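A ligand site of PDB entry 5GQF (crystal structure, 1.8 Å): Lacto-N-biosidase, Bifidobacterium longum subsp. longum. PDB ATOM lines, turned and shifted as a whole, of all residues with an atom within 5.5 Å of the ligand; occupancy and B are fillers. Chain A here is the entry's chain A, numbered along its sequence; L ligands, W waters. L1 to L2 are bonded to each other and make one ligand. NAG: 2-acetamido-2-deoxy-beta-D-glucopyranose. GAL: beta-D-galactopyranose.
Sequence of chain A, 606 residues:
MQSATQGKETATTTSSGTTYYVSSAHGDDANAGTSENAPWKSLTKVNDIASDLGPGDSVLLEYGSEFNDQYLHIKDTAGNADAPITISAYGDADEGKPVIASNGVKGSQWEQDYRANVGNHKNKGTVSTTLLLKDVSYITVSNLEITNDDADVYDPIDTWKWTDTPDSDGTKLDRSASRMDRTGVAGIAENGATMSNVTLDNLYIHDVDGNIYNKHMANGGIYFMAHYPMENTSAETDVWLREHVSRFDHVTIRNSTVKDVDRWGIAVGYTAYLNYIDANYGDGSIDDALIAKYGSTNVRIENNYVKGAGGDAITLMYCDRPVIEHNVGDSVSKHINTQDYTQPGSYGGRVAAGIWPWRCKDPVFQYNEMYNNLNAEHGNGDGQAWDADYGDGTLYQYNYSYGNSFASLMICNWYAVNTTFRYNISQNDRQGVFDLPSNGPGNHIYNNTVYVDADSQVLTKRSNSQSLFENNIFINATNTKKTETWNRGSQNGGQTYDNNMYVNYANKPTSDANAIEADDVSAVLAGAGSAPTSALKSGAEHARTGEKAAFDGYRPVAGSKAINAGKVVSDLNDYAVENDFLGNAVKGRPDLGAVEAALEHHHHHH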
ATOM      1  N   ASN A 120      25.308 -33.401 -12.740  1.00  0.00           N
ATOM      2  CA  ASN A 120      24.367 -33.494 -13.859  1.00  0.00           C
ATOM      3  C   ASN A 120      24.052 -32.139 -14.451  1.00  0.00           C
ATOM      4  O   ASN A 120      22.930 -31.589 -14.295  1.00  0.00           O
ATOM      5  CB  ASN A 120      23.098 -34.189 -13.450  1.00  0.00           C
ATOM      6  CG  ASN A 120      22.167 -34.459 -14.626  1.00  0.00           C
ATOM      7  OD1 ASN A 120      22.574 -34.454 -15.801  1.00  0.00           O
ATOM      8  ND2 ASN A 120      20.881 -34.679 -14.290  1.00  0.00           N
ATOM      9  N   HIS A 121      25.039 -31.599 -15.178  1.00  0.00           N
ATOM     10  CA  HIS A 121      24.958 -30.258 -15.731  1.00  0.00           C
ATOM     11  C   HIS A 121      25.809 -30.162 -17.026  1.00  0.00           C
ATOM     12  O   HIS A 121      26.749 -30.970 -17.247  1.00  0.00           O
ATOM     13  CB  HIS A 121      25.553 -29.244 -14.745  1.00  0.00           C
ATOM     14  CG  HIS A 121      24.885 -29.251 -13.417  1.00  0.00           C
ATOM     15  ND1 HIS A 121      23.679 -28.616 -13.193  1.00  0.00           N
ATOM     16  CD2 HIS A 121      25.235 -29.863 -12.248  1.00  0.00           C
ATOM     17  CE1 HIS A 121      23.324 -28.791 -11.934  1.00  0.00           C
ATOM     18  NE2 HIS A 121      24.249 -29.528 -11.333  1.00  0.00           N
ATOM     19  N   LYS A 215      23.199 -24.073 -15.007  1.00  0.00           N
ATOM     20  CA  LYS A 215      23.598 -23.629 -13.673  1.00  0.00           C
ATOM     21  C   LYS A 215      25.069 -23.444 -13.482  1.00  0.00           C
ATOM     22  O   LYS A 215      25.438 -22.685 -12.588  1.00  0.00           O
ATOM     23  CB  LYS A 215      23.093 -24.627 -12.632  1.00  0.00           C
ATOM     24  CG  LYS A 215      21.619 -24.457 -12.338  1.00  0.00           C
ATOM     25  CD  LYS A 215      21.150 -25.391 -11.195  1.00  0.00           C
ATOM     26  CE  LYS A 215      21.630 -24.957  -9.851  1.00  0.00           C
ATOM     27  NZ  LYS A 215      21.341 -26.047  -8.869  1.00  0.00           N
ATOM     28  N   HIS A 216      25.902 -24.109 -14.288  1.00  0.00           N
ATOM     29  CA  HIS A 216      27.381 -24.091 -14.006  1.00  0.00           C
ATOM     30  C   HIS A 216      28.282 -23.834 -15.213  1.00  0.00           C
ATOM     31  O   HIS A 216      29.524 -23.890 -15.074  1.00  0.00           O
ATOM     32  CB  HIS A 216      27.779 -25.364 -13.309  1.00  0.00           C
ATOM     33  CG  HIS A 216      27.073 -25.561 -12.017  1.00  0.00           C
ATOM     34  ND1 HIS A 216      27.337 -24.791 -10.923  1.00  0.00           N
ATOM     35  CD2 HIS A 216      26.034 -26.377 -11.682  1.00  0.00           C
ATOM     36  CE1 HIS A 216      26.528 -25.132  -9.938  1.00  0.00           C
ATOM     37  NE2 HIS A 216      25.747 -26.106 -10.341  1.00  0.00           N
ATOM     38  N   TRP A 264      22.367 -17.130 -13.340  1.00  0.00           N
ATOM     39  CA  TRP A 264      22.798 -16.733 -12.009  1.00  0.00           C
ATOM     40  C   TRP A 264      23.000 -15.220 -11.919  1.00  0.00           C
ATOM     41  O   TRP A 264      23.408 -14.607 -12.913  1.00  0.00           O
ATOM     42  CB  TRP A 264      24.089 -17.481 -11.587  1.00  0.00           C
ATOM     43  CG  TRP A 264      23.946 -18.067 -10.177  1.00  0.00           C
ATOM     44  CD1 TRP A 264      23.800 -17.413  -9.031  1.00  0.00           C
ATOM     45  CD2 TRP A 264      23.876 -19.438  -9.876  1.00  0.00           C
ATOM     46  NE1 TRP A 264      23.714 -18.275  -7.978  1.00  0.00           N
ATOM     47  CE2 TRP A 264      23.688 -19.554  -8.474  1.00  0.00           C
ATOM     48  CE3 TRP A 264      23.937 -20.575 -10.636  1.00  0.00           C
ATOM     49  CZ2 TRP A 264      23.518 -20.744  -7.854  1.00  0.00           C
ATOM     50  CZ3 TRP A 264      23.780 -21.791 -10.039  1.00  0.00           C
ATOM     51  CH2 TRP A 264      23.597 -21.896  -8.643  1.00  0.00           C
ATOM     52  N   TYR A 270      32.480 -22.567  -8.131  1.00  0.00           N
ATOM     53  CA  TYR A 270      32.282 -23.915  -8.697  1.00  0.00           C
ATOM     54  C   TYR A 270      33.578 -24.450  -9.356  1.00  0.00           C
ATOM     55  O   TYR A 270      34.266 -23.702 -10.041  1.00  0.00           O
ATOM     56  CB  TYR A 270      31.083 -23.957  -9.705  1.00  0.00           C
ATOM     57  CG  TYR A 270      30.402 -25.274  -9.732  1.00  0.00           C
ATOM     58  CD1 TYR A 270      29.655 -25.732  -8.617  1.00  0.00           C
ATOM     59  CD2 TYR A 270      30.452 -26.084 -10.861  1.00  0.00           C
ATOM     60  CE1 TYR A 270      29.007 -26.965  -8.686  1.00  0.00           C
ATOM     61  CE2 TYR A 270      29.785 -27.296 -10.919  1.00  0.00           C
ATOM     62  CZ  TYR A 270      29.076 -27.732  -9.765  1.00  0.00           C
ATOM     63  OH  TYR A 270      28.393 -28.938  -9.808  1.00  0.00           O
ATOM     64  N   ASP A 312      19.024 -18.013  -9.221  1.00  0.00           N
ATOM     65  CA  ASP A 312      19.508 -17.657  -7.879  1.00  0.00           C
ATOM     66  C   ASP A 312      20.191 -16.288  -7.862  1.00  0.00           C
ATOM     67  O   ASP A 312      20.706 -15.795  -8.908  1.00  0.00           O
ATOM     68  CB  ASP A 312      20.432 -18.716  -7.408  1.00  0.00           C
ATOM     69  CG  ASP A 312      19.786 -20.094  -7.267  1.00  0.00           C
ATOM     70  OD1 ASP A 312      19.761 -20.832  -8.315  1.00  0.00           O
ATOM     71  OD2 ASP A 312      19.514 -20.543  -6.114  1.00  0.00           O
ATOM     72  N   THR A 315      25.341 -16.994  -4.883  1.00  0.00           N
ATOM     73  CA  THR A 315      25.743 -18.281  -4.324  1.00  0.00           C
ATOM     74  C   THR A 315      27.258 -18.457  -4.241  1.00  0.00           C
ATOM     75  O   THR A 315      28.015 -18.144  -5.190  1.00  0.00           O
ATOM     76  CB  THR A 315      25.080 -19.421  -5.086  1.00  0.00           C
ATOM     77  OG1 THR A 315      23.685 -19.165  -5.199  1.00  0.00           O
ATOM     78  CG2 THR A 315      25.299 -20.797  -4.462  1.00  0.00           C
ATOM     79  N   MET A 317      30.196 -21.197  -3.749  1.00  0.00           N
ATOM     80  CA  MET A 317      30.426 -22.626  -3.950  1.00  0.00           C
ATOM     81  C   MET A 317      31.821 -23.059  -3.574  1.00  0.00           C
ATOM     82  O   MET A 317      32.834 -22.476  -4.088  1.00  0.00           O
ATOM     83  CB  MET A 317      30.172 -22.936  -5.434  1.00  0.00           C
ATOM     84  CG  MET A 317      28.742 -22.539  -5.921  1.00  0.00           C
ATOM     85  SD  MET A 317      28.575 -22.147  -7.663  1.00  0.00           S
ATOM     86  CE  MET A 317      26.779 -21.874  -7.887  1.00  0.00           C
ATOM     87  N   TYR A 318      31.927 -24.095  -2.758  1.00  0.00           N
ATOM     88  CA  TYR A 318      33.289 -24.699  -2.510  1.00  0.00           C
ATOM     89  C   TYR A 318      34.194 -23.597  -1.995  1.00  0.00           C
ATOM     90  O   TYR A 318      35.402 -23.580  -2.358  1.00  0.00           O
ATOM     91  CB  TYR A 318      33.909 -25.367  -3.759  1.00  0.00           C
ATOM     92  CG  TYR A 318      33.064 -26.509  -4.209  1.00  0.00           C
ATOM     93  CD1 TYR A 318      32.996 -27.672  -3.476  1.00  0.00           C
ATOM     94  CD2 TYR A 318      32.179 -26.367  -5.273  1.00  0.00           C
ATOM     95  CE1 TYR A 318      32.201 -28.718  -3.834  1.00  0.00           C
ATOM     96  CE2 TYR A 318      31.390 -27.406  -5.661  1.00  0.00           C
ATOM     97  CZ  TYR A 318      31.359 -28.571  -4.922  1.00  0.00           C
ATOM     98  OH  TYR A 318      30.519 -29.610  -5.283  1.00  0.00           O
ATOM     99  N   VAL A 351      14.482 -24.781  -9.914  1.00  0.00           N
ATOM    100  CA  VAL A 351      14.565 -24.451  -8.537  1.00  0.00           C
ATOM    101  C   VAL A 351      15.541 -23.335  -8.329  1.00  0.00           C
ATOM    102  O   VAL A 351      16.529 -23.290  -9.033  1.00  0.00           O
ATOM    103  CB  VAL A 351      15.008 -25.672  -7.689  1.00  0.00           C
ATOM    104  CG1 VAL A 351      13.875 -26.744  -7.622  1.00  0.00           C
ATOM    105  CG2 VAL A 351      16.257 -26.299  -8.154  1.00  0.00           C
ATOM    106  N   ALA A 352      15.255 -22.395  -7.439  1.00  0.00           N
ATOM    107  CA  ALA A 352      16.248 -21.364  -7.073  1.00  0.00           C
ATOM    108  C   ALA A 352      15.890 -20.772  -5.706  1.00  0.00           C
ATOM    109  O   ALA A 352      14.693 -20.610  -5.396  1.00  0.00           O
ATOM    110  CB  ALA A 352      16.362 -20.266  -8.091  1.00  0.00           C
ATOM    111  N   ALA A 353      16.940 -20.436  -4.960  1.00  0.00           N
ATOM    112  CA  ALA A 353      16.916 -19.752  -3.680  1.00  0.00           C
ATOM    113  C   ALA A 353      17.661 -18.394  -3.817  1.00  0.00           C
ATOM    114  O   ALA A 353      18.120 -18.039  -4.864  1.00  0.00           O
ATOM    115  CB  ALA A 353      17.556 -20.590  -2.550  1.00  0.00           C
ATOM    116  N   TRP A 356      23.003 -17.704  -0.755  1.00  0.00           N
ATOM    117  CA  TRP A 356      23.283 -19.001  -0.080  1.00  0.00           C
ATOM    118  C   TRP A 356      24.607 -19.709  -0.400  1.00  0.00           C
ATOM    119  O   TRP A 356      25.213 -19.401  -1.394  1.00  0.00           O
ATOM    120  CB  TRP A 356      22.132 -19.981  -0.322  1.00  0.00           C
ATOM    121  CG  TRP A 356      21.843 -20.325  -1.785  1.00  0.00           C
ATOM    122  CD1 TRP A 356      21.202 -19.588  -2.642  1.00  0.00           C
ATOM    123  CD2 TRP A 356      22.192 -21.524  -2.444  1.00  0.00           C
ATOM    124  NE1 TRP A 356      21.096 -20.245  -3.855  1.00  0.00           N
ATOM    125  CE2 TRP A 356      21.694 -21.452  -3.738  1.00  0.00           C
ATOM    126  CE3 TRP A 356      22.845 -22.661  -2.039  1.00  0.00           C
ATOM    127  CZ2 TRP A 356      21.788 -22.505  -4.650  1.00  0.00           C
ATOM    128  CZ3 TRP A 356      22.953 -23.748  -2.922  1.00  0.00           C
ATOM    129  CH2 TRP A 356      22.448 -23.642  -4.223  1.00  0.00           C
ATOM    130  N   TRP A 358      26.897 -23.437  -1.163  1.00  0.00           N
ATOM    131  CA  TRP A 358      26.979 -24.846  -1.583  1.00  0.00           C
ATOM    132  C   TRP A 358      28.367 -25.406  -1.263  1.00  0.00           C
ATOM    133  O   TRP A 358      29.411 -24.900  -1.802  1.00  0.00           O
ATOM    134  CB  TRP A 358      26.800 -24.998  -3.115  1.00  0.00           C
ATOM    135  CG  TRP A 358      27.070 -26.304  -3.616  1.00  0.00           C
ATOM    136  CD1 TRP A 358      28.166 -26.689  -4.300  1.00  0.00           C
ATOM    137  CD2 TRP A 358      26.213 -27.478  -3.553  1.00  0.00           C
ATOM    138  NE1 TRP A 358      28.104 -28.007  -4.624  1.00  0.00           N
ATOM    139  CE2 TRP A 358      26.911 -28.524  -4.186  1.00  0.00           C
ATOM    140  CE3 TRP A 358      24.903 -27.734  -2.979  1.00  0.00           C
ATOM    141  CZ2 TRP A 358      26.392 -29.813  -4.314  1.00  0.00           C
ATOM    142  CZ3 TRP A 358      24.413 -28.988  -3.082  1.00  0.00           C
ATOM    143  CH2 TRP A 358      25.130 -30.019  -3.755  1.00  0.00           C
ATOM    144  N   ASN A 380       8.584 -22.876  -9.326  1.00  0.00           N
ATOM    145  CA  ASN A 380       9.858 -22.807  -8.564  1.00  0.00           C
ATOM    146  C   ASN A 380       9.713 -23.831  -7.413  1.00  0.00           C
ATOM    147  O   ASN A 380       8.943 -23.590  -6.482  1.00  0.00           O
ATOM    148  CB  ASN A 380      10.148 -21.445  -8.067  1.00  0.00           C
ATOM    149  CG  ASN A 380      11.546 -21.338  -7.432  1.00  0.00           C
ATOM    150  OD1 ASN A 380      12.201 -22.379  -7.182  1.00  0.00           O
ATOM    151  ND2 ASN A 380      11.955 -20.149  -7.141  1.00  0.00           N
ATOM    152  N   ASP A 382      11.787 -24.388  -5.059  1.00  0.00           N
ATOM    153  CA  ASP A 382      12.312 -23.727  -3.893  1.00  0.00           C
ATOM    154  C   ASP A 382      11.667 -22.349  -3.732  1.00  0.00           C
ATOM    155  O   ASP A 382      10.454 -22.336  -3.574  1.00  0.00           O
ATOM    156  CB  ASP A 382      13.854 -23.792  -3.884  1.00  0.00           C
ATOM    157  CG  ASP A 382      14.321 -25.195  -3.612  1.00  0.00           C
ATOM    158  OD1 ASP A 382      14.006 -25.810  -2.551  1.00  0.00           O
ATOM    159  OD2 ASP A 382      14.961 -25.772  -4.461  1.00  0.00           O
ATOM    160  N   GLN A 384      13.107 -19.792  -1.461  1.00  0.00           N
ATOM    161  CA  GLN A 384      13.432 -19.278  -0.178  1.00  0.00           C
ATOM    162  C   GLN A 384      14.343 -18.051  -0.277  1.00  0.00           C
ATOM    163  O   GLN A 384      15.063 -17.866  -1.258  1.00  0.00           O
ATOM    164  CB  GLN A 384      14.191 -20.318   0.655  1.00  0.00           C
ATOM    165  CG  GLN A 384      13.589 -21.703   0.833  1.00  0.00           C
ATOM    166  CD  GLN A 384      13.945 -22.623  -0.306  1.00  0.00           C
ATOM    167  OE1 GLN A 384      14.633 -22.227  -1.246  1.00  0.00           O
ATOM    168  NE2 GLN A 384      13.454 -23.846  -0.254  1.00  0.00           N
ATOM    169  N   ASP A 387      19.223 -20.406   2.152  1.00  0.00           N
ATOM    170  CA  ASP A 387      19.349 -21.856   1.929  1.00  0.00           C
ATOM    171  C   ASP A 387      20.667 -22.371   2.462  1.00  0.00           C
ATOM    172  O   ASP A 387      21.639 -22.383   1.701  1.00  0.00           O
ATOM    173  CB  ASP A 387      19.192 -22.174   0.421  1.00  0.00           C
ATOM    174  CG  ASP A 387      19.526 -23.581   0.034  1.00  0.00           C
ATOM    175  OD1 ASP A 387      19.611 -24.491   0.930  1.00  0.00           O
ATOM    176  OD2 ASP A 387      19.772 -23.798  -1.202  1.00  0.00           O
ATOM    177  N   ASP A 389      22.372 -25.075   2.312  1.00  0.00           N
ATOM    178  CA  ASP A 389      22.396 -26.207   1.471  1.00  0.00           C
ATOM    179  C   ASP A 389      23.470 -27.188   1.897  1.00  0.00           C
ATOM    180  O   ASP A 389      24.037 -27.039   2.986  1.00  0.00           O
ATOM    181  CB  ASP A 389      22.538 -25.778  -0.063  1.00  0.00           C
ATOM    182  CG  ASP A 389      21.752 -26.715  -0.998  1.00  0.00           C
ATOM    183  OD1 ASP A 389      22.010 -27.951  -1.018  1.00  0.00           O
ATOM    184  OD2 ASP A 389      20.800 -26.246  -1.649  1.00  0.00           O
ATOM    185  N   TYR A 390      23.776 -28.185   1.090  1.00  0.00           N
ATOM    186  CA  TYR A 390      24.872 -29.066   1.448  1.00  0.00           C
ATOM    187  C   TYR A 390      26.095 -28.188   1.825  1.00  0.00           C
ATOM    188  O   TYR A 390      26.369 -27.207   1.158  1.00  0.00           O
ATOM    189  CB  TYR A 390      25.283 -29.934   0.272  1.00  0.00           C
ATOM    190  CG  TYR A 390      24.524 -31.150  -0.010  1.00  0.00           C
ATOM    191  CD1 TYR A 390      23.270 -31.394   0.531  1.00  0.00           C
ATOM    192  CD2 TYR A 390      25.014 -32.058  -0.992  1.00  0.00           C
ATOM    193  CE1 TYR A 390      22.585 -32.542   0.207  1.00  0.00           C
ATOM    194  CE2 TYR A 390      24.294 -33.179  -1.323  1.00  0.00           C
ATOM    195  CZ  TYR A 390      23.084 -33.429  -0.678  1.00  0.00           C
ATOM    196  OH  TYR A 390      22.307 -34.528  -0.929  1.00  0.00           O
ATOM    197  N   MET A 410      15.662 -22.419   4.049  1.00  0.00           N
ATOM    198  CA  MET A 410      15.816 -23.838   3.893  1.00  0.00           C
ATOM    199  C   MET A 410      17.110 -24.378   4.537  1.00  0.00           C
ATOM    200  O   MET A 410      18.166 -23.773   4.392  1.00  0.00           O
ATOM    201  CB  MET A 410      15.747 -24.256   2.387  1.00  0.00           C
ATOM    202  CG  MET A 410      15.988 -25.740   2.172  1.00  0.00           C
ATOM    203  SD  MET A 410      15.612 -26.440   0.526  1.00  0.00           S
ATOM    204  CE  MET A 410      16.738 -25.564  -0.569  1.00  0.00           C
ATOM    205  N   CYS A 412      18.988 -27.908   3.679  1.00  0.00           N
ATOM    206  CA  CYS A 412      18.687 -28.835   2.562  1.00  0.00           C
ATOM    207  C   CYS A 412      19.324 -30.251   2.583  1.00  0.00           C
ATOM    208  O   CYS A 412      20.517 -30.426   2.180  1.00  0.00           O
ATOM    209  CB  CYS A 412      19.021 -28.198   1.169  1.00  0.00           C
ATOM    210  SG  CYS A 412      18.263 -29.248  -0.126  1.00  0.00           S
ATOM    211  N   ASN A 413      18.544 -31.262   3.018  1.00  0.00           N
ATOM    212  CA  ASN A 413      18.879 -32.675   2.782  1.00  0.00           C
ATOM    213  C   ASN A 413      20.114 -33.118   3.584  1.00  0.00           C
ATOM    214  O   ASN A 413      20.661 -32.342   4.371  1.00  0.00           O
ATOM    215  CB  ASN A 413      19.030 -33.009   1.250  1.00  0.00           C
ATOM    216  CG  ASN A 413      17.694 -33.131   0.471  1.00  0.00           C
ATOM    217  OD1 ASN A 413      16.594 -33.248   1.000  1.00  0.00           O
ATOM    218  ND2 ASN A 413      17.844 -33.072  -0.843  1.00  0.00           N
HETATM  219  C1  NAG L   1      18.554 -27.269  -3.227  1.00  0.00           C
HETATM  220  C2  NAG L   1      19.474 -28.025  -4.158  1.00  0.00           C
HETATM  221  C3  NAG L   1      20.359 -27.053  -4.992  1.00  0.00           C
HETATM  222  C4  NAG L   1      19.552 -25.927  -5.619  1.00  0.00           C
HETATM  223  C5  NAG L   1      18.919 -25.202  -4.431  1.00  0.00           C
HETATM  224  C6  NAG L   1      18.220 -23.889  -4.777  1.00  0.00           C
HETATM  225  C7  NAG L   1      20.213 -30.198  -3.307  1.00  0.00           C
HETATM  226  C8  NAG L   1      21.071 -30.908  -2.282  1.00  0.00           C
HETATM  227  N2  NAG L   1      20.297 -28.870  -3.321  1.00  0.00           N
HETATM  228  O1  NAG L   1      17.433 -28.144  -2.855  1.00  0.00           O
HETATM  229  O3  NAG L   1      20.845 -27.806  -6.070  1.00  0.00           O
HETATM  230  O4  NAG L   1      20.381 -25.029  -6.459  1.00  0.00           O
HETATM  231  O5  NAG L   1      17.995 -26.122  -3.833  1.00  0.00           O
HETATM  232  O6  NAG L   1      17.101 -24.136  -5.696  1.00  0.00           O
HETATM  233  O7  NAG L   1      19.500 -30.778  -4.102  1.00  0.00           O
HETATM  234  C1  GAL L   2      22.210 -28.119  -6.088  1.00  0.00           C
HETATM  235  C2  GAL L   2      22.508 -29.271  -7.083  1.00  0.00           C
HETATM  236  C3  GAL L   2      23.995 -29.402  -7.438  1.00  0.00           C
HETATM  237  C4  GAL L   2      24.545 -28.008  -7.783  1.00  0.00           C
HETATM  238  C5  GAL L   2      24.279 -27.073  -6.612  1.00  0.00           C
HETATM  239  C6  GAL L   2      24.870 -25.704  -6.796  1.00  0.00           C
HETATM  240  O2  GAL L   2      21.980 -30.539  -6.674  1.00  0.00           O
HETATM  241  O3  GAL L   2      24.088 -30.346  -8.532  1.00  0.00           O
HETATM  242  O4  GAL L   2      23.895 -27.418  -8.912  1.00  0.00           O
HETATM  243  O5  GAL L   2      22.855 -26.928  -6.344  1.00  0.00           O
HETATM  244  O6  GAL L   2      26.322 -25.787  -6.808  1.00  0.00           O
HETATM  245  O   HOH W   1      24.330 -33.391 -10.203  1.00  0.00           O
HETATM  246  O   HOH W   2      22.182 -32.198  -9.803  1.00  0.00           O
HETATM  247  O   HOH W   3      19.429 -33.486  -3.985  1.00  0.00           O
HETATM  248  O   HOH W   4      19.208 -23.361  -8.043  1.00  0.00           O
HETATM  249  O   HOH W   5      19.509 -30.957  -6.726  1.00  0.00           O
HETATM  250  O   HOH W   6      23.146 -32.492  -5.403  1.00  0.00           O
HETATM  251  O   HOH W   7      15.328 -28.362  -4.353  1.00  0.00           O
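An oxygen (O4) of NAG L1 sits at hydrogen-bond distance from the side-chain amino group (NZ) of Lys 215. N of Ala 352 sits at hydrogen-bond distance from O6 of NAG L1, at 3.1 Å. The side-chain sulfur (SG) of Cys 412 lies within hydrogen-bond range of an oxygen (O1) of NAG L1 (3.1 Å). OD1 of Asp 389 lies within hydrogen-bond range of N2 of NAG L1 (3.0 Å). The backbone carbonyl oxygen (O) of Val 351 sits close to an oxygen (O6) of NAG L1 (3.5 Å). O6 of NAG L1 lies within hydrogen-bond range of OD2 of Asp 382. A ring nitrogen (NE2) of His 121 is in hydrogen-bond range of an oxygen (O3) of GAL L2 (2.9 Å). O4 of GAL L2 sits at hydrogen-bond distance from NE2 of His 216, at 2.7 Å.
The backbone NH (N) of Tyr 318 sits at hydrogen-bond distance from the backbone carbonyl oxygen (O) of Trp 358 (2.8 Å). NE2 of Gln 384 is in hydrogen-bond range of SD of Met 410 (3.5 Å). OD1 of Asp 382 lies within hydrogen-bond range of NE2 of Gln 384, at 3.1 Å. N of Asp 382 is in hydrogen-bond range of OD1 of Asn 380 (3.0 Å). The side-chain carboxylate (OD1) of Asp 387 is in hydrogen-bond range of the backbone NH (N) of Asp 389. The backbone NH of Ala 352 lies within hydrogen-bond range of the side-chain amide oxygen of Asn 380. The indole nitrogen (NE1) of Trp 356 lies within hydrogen-bond range of the side-chain hydroxyl (OG1) of Thr 315, at 3.1 Å. NE1 of Trp 356 sits at hydrogen-bond distance from OD2 of Asp 312.
Residues that only touch the ligand: Trp 358, Tyr 390, Trp 356, Tyr 270, Met 410, Asp 387, Ala 353 and Asp 312. Hydrophobic or aromatic side chains that line the ligand: His 121, His 216, Tyr 270, Val 351, Trp 356, Trp 358, Tyr 390 and Met 410. Of the 24 residues printed, 16 come within 4 Å of the ligand.
Water W4 lies within hydrogen-bond range of an oxygen (O4) of NAG L1 (2.6 Å), the side-chain carboxylate of Asp 312 (2.6 Å) and the backbone carbonyl oxygen of Val 351 (2.9 Å). Water W7 bridges an oxygen (O1) of NAG L1 (2.6 Å) and the side-chain carboxylate (OD2) of Asp 382 (2.6 Å). Water W1 lies within hydrogen-bond range of N of Asn 120 (2.7 Å) and O3 of GAL L2 (3.5 Å).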
